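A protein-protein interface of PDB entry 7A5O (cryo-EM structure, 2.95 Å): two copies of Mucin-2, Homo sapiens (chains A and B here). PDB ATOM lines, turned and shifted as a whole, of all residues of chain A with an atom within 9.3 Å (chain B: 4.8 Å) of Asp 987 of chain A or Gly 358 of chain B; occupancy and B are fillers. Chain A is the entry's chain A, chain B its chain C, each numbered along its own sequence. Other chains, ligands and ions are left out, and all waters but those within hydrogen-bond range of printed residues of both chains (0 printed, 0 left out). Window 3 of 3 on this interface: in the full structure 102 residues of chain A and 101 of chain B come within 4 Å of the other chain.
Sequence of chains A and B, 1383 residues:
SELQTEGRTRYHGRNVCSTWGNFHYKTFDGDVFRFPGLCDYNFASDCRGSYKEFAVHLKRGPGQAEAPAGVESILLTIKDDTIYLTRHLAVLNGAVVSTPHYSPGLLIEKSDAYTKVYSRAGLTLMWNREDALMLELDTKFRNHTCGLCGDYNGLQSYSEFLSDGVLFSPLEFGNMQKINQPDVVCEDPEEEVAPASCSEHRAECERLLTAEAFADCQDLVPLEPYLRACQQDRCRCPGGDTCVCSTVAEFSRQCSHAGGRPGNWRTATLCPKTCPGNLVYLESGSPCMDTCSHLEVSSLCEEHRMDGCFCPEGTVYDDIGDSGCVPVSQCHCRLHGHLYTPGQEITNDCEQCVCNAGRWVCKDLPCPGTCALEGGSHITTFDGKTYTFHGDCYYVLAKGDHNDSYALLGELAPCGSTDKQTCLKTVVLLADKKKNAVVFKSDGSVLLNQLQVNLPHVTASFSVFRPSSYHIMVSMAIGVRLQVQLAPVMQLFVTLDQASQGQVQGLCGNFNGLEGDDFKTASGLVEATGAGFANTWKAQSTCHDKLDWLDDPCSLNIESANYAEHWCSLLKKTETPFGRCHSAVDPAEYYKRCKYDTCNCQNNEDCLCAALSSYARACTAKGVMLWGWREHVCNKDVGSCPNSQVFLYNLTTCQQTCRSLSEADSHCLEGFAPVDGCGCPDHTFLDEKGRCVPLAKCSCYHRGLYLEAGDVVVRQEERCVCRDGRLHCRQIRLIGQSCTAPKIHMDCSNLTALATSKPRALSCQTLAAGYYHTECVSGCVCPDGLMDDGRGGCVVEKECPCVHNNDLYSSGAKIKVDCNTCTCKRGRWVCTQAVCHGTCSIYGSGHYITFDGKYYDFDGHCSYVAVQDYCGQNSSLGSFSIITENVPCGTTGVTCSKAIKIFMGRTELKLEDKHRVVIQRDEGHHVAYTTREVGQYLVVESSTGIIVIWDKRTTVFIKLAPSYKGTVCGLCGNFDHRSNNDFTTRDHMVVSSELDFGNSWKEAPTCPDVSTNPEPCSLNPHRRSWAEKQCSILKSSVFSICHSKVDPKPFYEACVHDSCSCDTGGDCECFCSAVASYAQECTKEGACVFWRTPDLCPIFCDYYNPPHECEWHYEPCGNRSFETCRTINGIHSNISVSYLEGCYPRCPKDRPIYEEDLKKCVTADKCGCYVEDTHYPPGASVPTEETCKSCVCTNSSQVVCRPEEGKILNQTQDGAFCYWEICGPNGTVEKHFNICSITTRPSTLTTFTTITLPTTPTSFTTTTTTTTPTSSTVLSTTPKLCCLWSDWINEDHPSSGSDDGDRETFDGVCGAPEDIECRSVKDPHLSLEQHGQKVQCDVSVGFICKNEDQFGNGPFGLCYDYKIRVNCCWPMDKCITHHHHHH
Arg 334 of chain B touches Asp 987 of chain A.
Asp 987 of chain A touches Gly 358 of chain B (CB to O, 3.9 Å).
CA of Arg 359 of chain B touches O of Asp 987 of chain A (3.9 Å).
Arg 359 of chain B touches His 988 of chain A.
O of Trp 360 of chain B touches CB of His 988 of chain A, at 3.7 Å.
Asp 987 of chain A touches four residues of chain B.
Gly 358 of chain B touches just one residue of chain A: Asp 987 (3.9 Å).
Cys 331 of chain B touches none of the printed residues of chain A.
No residue of chain A comes within 4 Å of Ala 357 of chain B.
Printed residues of chain A within 4 Å of Arg 359 of chain B: Asp 987 and His 988.
Of the printed residues of chain A, Trp 360 of chain B touches Asp 987 (3.0 Å) and His 988 (3.7 Å).
Printed residues of chain B within 4 Å of His 988 of chain A: Arg 359 (3.2 Å) and Trp 360 (3.7 Å).
The nearest printed residue of chain B that does not touch Asp 987 of chain A is Cys 333 of chain B (5.6 Å).
The nearest printed residue of chain A that does not touch Arg 359 of chain B is Arg 986 of chain A (5.6 Å).
No position is printed for both chains.
Of the 6 pairs that touch across the chains among the printed residues, none has its exchanged pair printed and touching as well.
Of the 9 printed residues of chain B, 4 touch a printed residue of chain A.
Printed residues of chain B that touch a printed residue of chain A: Arg 334, Gly 358, Arg 359 and Trp 360.
Hydrophobic or aromatic side chains of chain A within 4 Å of the printed part of chain B: His 988.
Among the printed residues, no Asp or Glu carboxylate lies within 4 Å of a Lys or Arg side-chain nitrogen of the other chain.
O of Asp 987 of chain A sits at hydrogen-bond distance from N of Trp 360 of chain B.
SG of Cys 292 of chain B forms a disulfide with SG of Cys 331 of chain B, at 2.0 Å.
The side-chain sulfur (SG) of Cys 871 of chain A is disulfide-bonded to the side-chain sulfur (SG) of Cys 969 of chain A, at 2.0 Å.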
ATOM      1  N   CYS A 871      16.126  11.306  22.212  1.00  0.00           N
ATOM      2  CA  CYS A 871      15.397  11.032  20.978  1.00  0.00           C
ATOM      3  C   CYS A 871      16.155   9.956  20.218  1.00  0.00           C
ATOM      4  O   CYS A 871      16.905  10.254  19.289  1.00  0.00           O
ATOM      5  CB  CYS A 871      15.249  12.309  20.139  1.00  0.00           C
ATOM      6  SG  CYS A 871      14.339  13.664  20.929  1.00  0.00           S
ATOM      7  N   GLY A 872      15.946   8.705  20.599  1.00  0.00           N
ATOM      8  CA  GLY A 872      16.597   7.591  19.935  1.00  0.00           C
ATOM      9  C   GLY A 872      18.078   7.470  20.228  1.00  0.00           C
ATOM     10  O   GLY A 872      18.916   7.659  19.349  1.00  0.00           O
ATOM     11  N   CYS A 969      12.994  16.409  20.157  1.00  0.00           N
ATOM     12  CA  CYS A 969      11.730  15.830  19.708  1.00  0.00           C
ATOM     13  C   CYS A 969      10.678  16.096  20.774  1.00  0.00           C
ATOM     14  O   CYS A 969      10.958  16.707  21.805  1.00  0.00           O
ATOM     15  CB  CYS A 969      11.865  14.335  19.395  1.00  0.00           C
ATOM     16  SG  CYS A 969      12.366  13.256  20.732  1.00  0.00           S
ATOM     17  N   PHE A 983       5.489  16.176  12.614  1.00  0.00           N
ATOM     18  CA  PHE A 983       4.649  15.107  13.143  1.00  0.00           C
ATOM     19  C   PHE A 983       5.353  13.760  13.076  1.00  0.00           C
ATOM     20  O   PHE A 983       4.833  12.796  12.546  1.00  0.00           O
ATOM     21  CB  PHE A 983       3.304  15.050  12.431  1.00  0.00           C
ATOM     22  CG  PHE A 983       2.371  16.190  12.749  1.00  0.00           C
ATOM     23  CD1 PHE A 983       2.677  17.127  13.718  1.00  0.00           C
ATOM     24  CD2 PHE A 983       1.134  16.257  12.148  1.00  0.00           C
ATOM     25  CE1 PHE A 983       1.814  18.135  14.018  1.00  0.00           C
ATOM     26  CE2 PHE A 983       0.261  17.272  12.458  1.00  0.00           C
ATOM     27  CZ  PHE A 983       0.603  18.201  13.398  1.00  0.00           C
ATOM     28  N   THR A 984       6.549  13.694  13.644  1.00  0.00           N
ATOM     29  CA  THR A 984       7.259  12.442  13.847  1.00  0.00           C
ATOM     30  C   THR A 984       6.854  11.874  15.198  1.00  0.00           C
ATOM     31  O   THR A 984       6.917  12.573  16.209  1.00  0.00           O
ATOM     32  CB  THR A 984       8.770  12.655  13.802  1.00  0.00           C
ATOM     33  OG1 THR A 984       9.138  13.216  12.543  1.00  0.00           O
ATOM     34  CG2 THR A 984       9.482  11.348  13.956  1.00  0.00           C
ATOM     35  N   THR A 985       6.444  10.611  15.217  1.00  0.00           N
ATOM     36  CA  THR A 985       5.987   9.997  16.448  1.00  0.00           C
ATOM     37  C   THR A 985       7.181   9.499  17.259  1.00  0.00           C
ATOM     38  O   THR A 985       8.336   9.689  16.883  1.00  0.00           O
ATOM     39  CB  THR A 985       4.999   8.879  16.137  1.00  0.00           C
ATOM     40  OG1 THR A 985       5.639   7.891  15.327  1.00  0.00           O
ATOM     41  CG2 THR A 985       3.811   9.418  15.387  1.00  0.00           C
ATOM     42  N   ARG A 986       6.898   8.875  18.407  1.00  0.00           N
ATOM     43  CA  ARG A 986       7.953   8.376  19.284  1.00  0.00           C
ATOM     44  C   ARG A 986       8.747   7.246  18.635  1.00  0.00           C
ATOM     45  O   ARG A 986       9.941   7.091  18.906  1.00  0.00           O
ATOM     46  CB  ARG A 986       7.350   7.926  20.617  1.00  0.00           C
ATOM     47  CG  ARG A 986       8.366   7.537  21.678  1.00  0.00           C
ATOM     48  CD  ARG A 986       7.752   7.006  22.958  1.00  0.00           C
ATOM     49  NE  ARG A 986       7.049   7.969  23.797  1.00  0.00           N
ATOM     50  CZ  ARG A 986       7.630   8.706  24.735  1.00  0.00           C
ATOM     51  NH1 ARG A 986       8.929   8.604  24.951  1.00  0.00           N
ATOM     52  NH2 ARG A 986       6.915   9.533  25.469  1.00  0.00           N
ATOM     53  N   ASP A 987       8.125   6.475  17.748  1.00  0.00           N
ATOM     54  CA  ASP A 987       8.809   5.410  17.025  1.00  0.00           C
ATOM     55  C   ASP A 987       9.342   5.851  15.666  1.00  0.00           C
ATOM     56  O   ASP A 987       9.465   5.010  14.773  1.00  0.00           O
ATOM     57  CB  ASP A 987       7.889   4.202  16.875  1.00  0.00           C
ATOM     58  CG  ASP A 987       6.591   4.528  16.165  1.00  0.00           C
ATOM     59  OD1 ASP A 987       6.328   5.709  15.862  1.00  0.00           O
ATOM     60  OD2 ASP A 987       5.823   3.579  15.902  1.00  0.00           O
ATOM     61  N   HIS A 988       9.615   7.151  15.496  1.00  0.00           N
ATOM     62  CA  HIS A 988      10.335   7.724  14.353  1.00  0.00           C
ATOM     63  C   HIS A 988       9.585   7.535  13.037  1.00  0.00           C
ATOM     64  O   HIS A 988      10.150   7.126  12.025  1.00  0.00           O
ATOM     65  CB  HIS A 988      11.750   7.162  14.259  1.00  0.00           C
ATOM     66  CG  HIS A 988      12.620   7.523  15.417  1.00  0.00           C
ATOM     67  ND1 HIS A 988      13.200   8.762  15.551  1.00  0.00           N
ATOM     68  CD2 HIS A 988      13.008   6.806  16.496  1.00  0.00           C
ATOM     69  CE1 HIS A 988      13.917   8.789  16.658  1.00  0.00           C
ATOM     70  NE2 HIS A 988      13.817   7.614  17.250  1.00  0.00           N
ATOM     71  N   MET A 989       8.301   7.857  13.054  1.00  0.00           N
ATOM     72  CA  MET A 989       7.420   7.726  11.905  1.00  0.00           C
ATOM     73  C   MET A 989       6.661   9.023  11.702  1.00  0.00           C
ATOM     74  O   MET A 989       5.997   9.501  12.622  1.00  0.00           O
ATOM     75  CB  MET A 989       6.447   6.568  12.110  1.00  0.00           C
ATOM     76  CG  MET A 989       5.459   6.345  10.993  1.00  0.00           C
ATOM     77  SD  MET A 989       6.123   5.840   9.410  1.00  0.00           S
ATOM     78  CE  MET A 989       4.817   6.455   8.355  1.00  0.00           C
ATOM     79  N   VAL A 990       6.753   9.590  10.506  1.00  0.00           N
ATOM     80  CA  VAL A 990       6.053  10.827  10.187  1.00  0.00           C
ATOM     81  C   VAL A 990       4.636  10.469   9.761  1.00  0.00           C
ATOM     82  O   VAL A 990       4.429   9.851   8.716  1.00  0.00           O
ATOM     83  CB  VAL A 990       6.774  11.629   9.101  1.00  0.00           C
ATOM     84  CG1 VAL A 990       5.975  12.847   8.758  1.00  0.00           C
ATOM     85  CG2 VAL A 990       8.125  12.049   9.582  1.00  0.00           C
ATOM     86  N   VAL A 991       3.660  10.860  10.571  1.00  0.00           N
ATOM     87  CA  VAL A 991       2.256  10.632  10.283  1.00  0.00           C
ATOM     88  C   VAL A 991       1.628  11.956   9.862  1.00  0.00           C
ATOM     89  O   VAL A 991       2.236  13.017   9.973  1.00  0.00           O
ATOM     90  CB  VAL A 991       1.515  10.014  11.481  1.00  0.00           C
ATOM     91  CG1 VAL A 991       2.087   8.652  11.797  1.00  0.00           C
ATOM     92  CG2 VAL A 991       1.620  10.903  12.685  1.00  0.00           C
ATOM     93  N   ASP A 996      -2.630  10.875  15.982  1.00  0.00           N
ATOM     94  CA  ASP A 996      -1.680   9.776  16.073  1.00  0.00           C
ATOM     95  C   ASP A 996      -0.320  10.244  16.540  1.00  0.00           C
ATOM     96  O   ASP A 996       0.405   9.475  17.169  1.00  0.00           O
ATOM     97  CB  ASP A 996      -1.513   9.088  14.720  1.00  0.00           C
ATOM     98  CG  ASP A 996      -2.727   8.304  14.307  1.00  0.00           C
ATOM     99  OD1 ASP A 996      -3.460   7.808  15.184  1.00  0.00           O
ATOM    100  OD2 ASP A 996      -2.941   8.172  13.090  1.00  0.00           O
ATOM    101  N   PHE A 997       0.037  11.482  16.205  1.00  0.00           N
ATOM    102  CA  PHE A 997       1.261  12.109  16.693  1.00  0.00           C
ATOM    103  C   PHE A 997       1.178  12.449  18.171  1.00  0.00           C
ATOM    104  O   PHE A 997       2.058  12.069  18.946  1.00  0.00           O
ATOM    105  CB  PHE A 997       1.550  13.341  15.839  1.00  0.00           C
ATOM    106  CG  PHE A 997       2.585  14.266  16.394  1.00  0.00           C
ATOM    107  CD1 PHE A 997       3.908  13.918  16.471  1.00  0.00           C
ATOM    108  CD2 PHE A 997       2.220  15.545  16.767  1.00  0.00           C
ATOM    109  CE1 PHE A 997       4.827  14.806  16.969  1.00  0.00           C
ATOM    110  CE2 PHE A 997       3.143  16.426  17.253  1.00  0.00           C
ATOM    111  CZ  PHE A 997       4.440  16.057  17.353  1.00  0.00           C
ATOM    112  N   ASN A 999      -0.906  11.403  20.521  1.00  0.00           N
ATOM    113  CA  ASN A 999      -1.128  10.257  21.391  1.00  0.00           C
ATOM    114  C   ASN A 999       0.102   9.389  21.573  1.00  0.00           C
ATOM    115  O   ASN A 999       0.067   8.468  22.388  1.00  0.00           O
ATOM    116  CB  ASN A 999      -2.262   9.377  20.867  1.00  0.00           C
ATOM    117  CG  ASN A 999      -3.628   9.979  21.091  1.00  0.00           C
ATOM    118  OD1 ASN A 999      -3.905  10.543  22.142  1.00  0.00           O
ATOM    119  ND2 ASN A 999      -4.501   9.836  20.112  1.00  0.00           N
ATOM    120  N   SER A1000       1.177   9.638  20.848  1.00  0.00           N
ATOM    121  CA  SER A1000       2.388   8.854  20.995  1.00  0.00           C
ATOM    122  C   SER A1000       3.389   9.482  21.943  1.00  0.00           C
ATOM    123  O   SER A1000       4.405   8.859  22.242  1.00  0.00           O
ATOM    124  CB  SER A1000       3.036   8.629  19.637  1.00  0.00           C
ATOM    125  OG  SER A1000       3.443   9.848  19.076  1.00  0.00           O
ATOM    126  N   TRP A1001       3.136  10.695  22.423  1.00  0.00           N
ATOM    127  CA  TRP A1001       4.046  11.346  23.347  1.00  0.00           C
ATOM    128  C   TRP A1001       3.500  11.389  24.762  1.00  0.00           C
ATOM    129  O   TRP A1001       4.042  12.112  25.593  1.00  0.00           O
ATOM    130  CB  TRP A1001       4.407  12.755  22.875  1.00  0.00           C
ATOM    131  CG  TRP A1001       5.236  12.749  21.646  1.00  0.00           C
ATOM    132  CD1 TRP A1001       4.836  13.039  20.383  1.00  0.00           C
ATOM    133  CD2 TRP A1001       6.593  12.337  21.550  1.00  0.00           C
ATOM    134  NE1 TRP A1001       5.873  12.879  19.514  1.00  0.00           N
ATOM    135  CE2 TRP A1001       6.963  12.436  20.209  1.00  0.00           C
ATOM    136  CE3 TRP A1001       7.537  11.903  22.477  1.00  0.00           C
ATOM    137  CZ2 TRP A1001       8.236  12.126  19.772  1.00  0.00           C
ATOM    138  CZ3 TRP A1001       8.795  11.596  22.044  1.00  0.00           C
ATOM    139  CH2 TRP A1001       9.135  11.704  20.706  1.00  0.00           C
ATOM    140  N   CYS B 292       9.697  -1.193  25.732  1.00  0.00           N
ATOM    141  CA  CYS B 292       9.747  -1.577  24.309  1.00  0.00           C
ATOM    142  C   CYS B 292       9.061  -0.602  23.338  1.00  0.00           C
ATOM    143  O   CYS B 292       9.260  -0.688  22.124  1.00  0.00           O
ATOM    144  CB  CYS B 292       9.176  -3.002  24.166  1.00  0.00           C
ATOM    145  SG  CYS B 292       8.955  -3.808  22.566  1.00  0.00           S
ATOM    146  N   CYS B 331      10.917  -6.666  19.452  1.00  0.00           N
ATOM    147  CA  CYS B 331       9.824  -5.708  19.590  1.00  0.00           C
ATOM    148  C   CYS B 331       9.070  -5.551  18.280  1.00  0.00           C
ATOM    149  O   CYS B 331       9.606  -5.036  17.295  1.00  0.00           O
ATOM    150  CB  CYS B 331      10.363  -4.364  20.067  1.00  0.00           C
ATOM    151  SG  CYS B 331      10.782  -4.275  21.815  1.00  0.00           S
ATOM    152  N   CYS B 333       6.573  -3.751  15.890  1.00  0.00           N
ATOM    153  CA  CYS B 333       6.152  -2.373  15.723  1.00  0.00           C
ATOM    154  C   CYS B 333       4.635  -2.312  15.620  1.00  0.00           C
ATOM    155  O   CYS B 333       3.948  -3.335  15.633  1.00  0.00           O
ATOM    156  CB  CYS B 333       6.799  -1.773  14.480  1.00  0.00           C
ATOM    157  SG  CYS B 333       8.594  -1.671  14.502  1.00  0.00           S
ATOM    158  N   ARG B 334       4.091  -1.105  15.507  1.00  0.00           N
ATOM    159  CA  ARG B 334       2.676  -0.973  15.210  1.00  0.00           C
ATOM    160  C   ARG B 334       2.463   0.293  14.402  1.00  0.00           C
ATOM    161  O   ARG B 334       3.250   1.239  14.473  1.00  0.00           O
ATOM    162  CB  ARG B 334       1.805  -0.953  16.474  1.00  0.00           C
ATOM    163  CG  ARG B 334       1.880   0.301  17.310  1.00  0.00           C
ATOM    164  CD  ARG B 334       1.029   0.155  18.569  1.00  0.00           C
ATOM    165  NE  ARG B 334       0.902   1.408  19.314  1.00  0.00           N
ATOM    166  CZ  ARG B 334       1.742   1.833  20.252  1.00  0.00           C
ATOM    167  NH1 ARG B 334       2.799   1.105  20.590  1.00  0.00           N
ATOM    168  NH2 ARG B 334       1.520   2.987  20.857  1.00  0.00           N
ATOM    169  N   ASN B 356      12.491  -1.886  12.628  1.00  0.00           N
ATOM    170  CA  ASN B 356      13.704  -2.274  13.328  1.00  0.00           C
ATOM    171  C   ASN B 356      13.290  -2.628  14.763  1.00  0.00           C
ATOM    172  O   ASN B 356      12.117  -2.912  15.015  1.00  0.00           O
ATOM    173  CB  ASN B 356      14.740  -1.153  13.199  1.00  0.00           C
ATOM    174  CG  ASN B 356      16.144  -1.604  13.540  1.00  0.00           C
ATOM    175  OD1 ASN B 356      16.366  -2.760  13.889  1.00  0.00           O
ATOM    176  ND2 ASN B 356      17.097  -0.686  13.449  1.00  0.00           N
ATOM    177  N   ALA B 357      14.223  -2.655  15.714  1.00  0.00           N
ATOM    178  CA  ALA B 357      13.930  -3.094  17.079  1.00  0.00           C
ATOM    179  C   ALA B 357      13.086  -2.040  17.789  1.00  0.00           C
ATOM    180  O   ALA B 357      13.577  -1.213  18.558  1.00  0.00           O
ATOM    181  CB  ALA B 357      15.222  -3.363  17.835  1.00  0.00           C
ATOM    182  N   GLY B 358      11.780  -2.083  17.526  1.00  0.00           N
ATOM    183  CA  GLY B 358      10.826  -1.208  18.159  1.00  0.00           C
ATOM    184  C   GLY B 358      10.563   0.092  17.432  1.00  0.00           C
ATOM    185  O   GLY B 358       9.482   0.664  17.593  1.00  0.00           O
ATOM    186  N   ARG B 359      11.512   0.574  16.640  1.00  0.00           N
ATOM    187  CA  ARG B 359      11.388   1.831  15.928  1.00  0.00           C
ATOM    188  C   ARG B 359      11.413   1.585  14.428  1.00  0.00           C
ATOM    189  O   ARG B 359      11.890   0.552  13.954  1.00  0.00           O
ATOM    190  CB  ARG B 359      12.511   2.795  16.317  1.00  0.00           C
ATOM    191  CG  ARG B 359      13.889   2.283  15.957  1.00  0.00           C
ATOM    192  CD  ARG B 359      14.972   3.267  16.343  1.00  0.00           C
ATOM    193  NE  ARG B 359      14.910   4.475  15.532  1.00  0.00           N
ATOM    194  CZ  ARG B 359      15.497   4.613  14.350  1.00  0.00           C
ATOM    195  NH1 ARG B 359      16.207   3.616  13.846  1.00  0.00           N
ATOM    196  NH2 ARG B 359      15.385   5.744  13.674  1.00  0.00           N
ATOM    197  N   TRP B 360      10.883   2.552  13.684  1.00  0.00           N
ATOM    198  CA  TRP B 360      10.846   2.488  12.233  1.00  0.00           C
ATOM    199  C   TRP B 360      12.064   3.181  11.642  1.00  0.00           C
ATOM    200  O   TRP B 360      12.503   4.219  12.140  1.00  0.00           O
ATOM    201  CB  TRP B 360       9.582   3.146  11.691  1.00  0.00           C
ATOM    202  CG  TRP B 360       8.324   2.444  12.010  1.00  0.00           C
ATOM    203  CD1 TRP B 360       7.456   2.743  13.005  1.00  0.00           C
ATOM    204  CD2 TRP B 360       7.767   1.324  11.315  1.00  0.00           C
ATOM    205  NE1 TRP B 360       6.391   1.884  12.983  1.00  0.00           N
ATOM    206  CE2 TRP B 360       6.560   1.000  11.951  1.00  0.00           C
ATOM    207  CE3 TRP B 360       8.175   0.564  10.217  1.00  0.00           C
ATOM    208  CZ2 TRP B 360       5.754  -0.050  11.526  1.00  0.00           C
ATOM    209  CZ3 TRP B 360       7.373  -0.478   9.799  1.00  0.00           C
ATOM    210  CH2 TRP B 360       6.179  -0.776  10.452  1.00  0.00           C
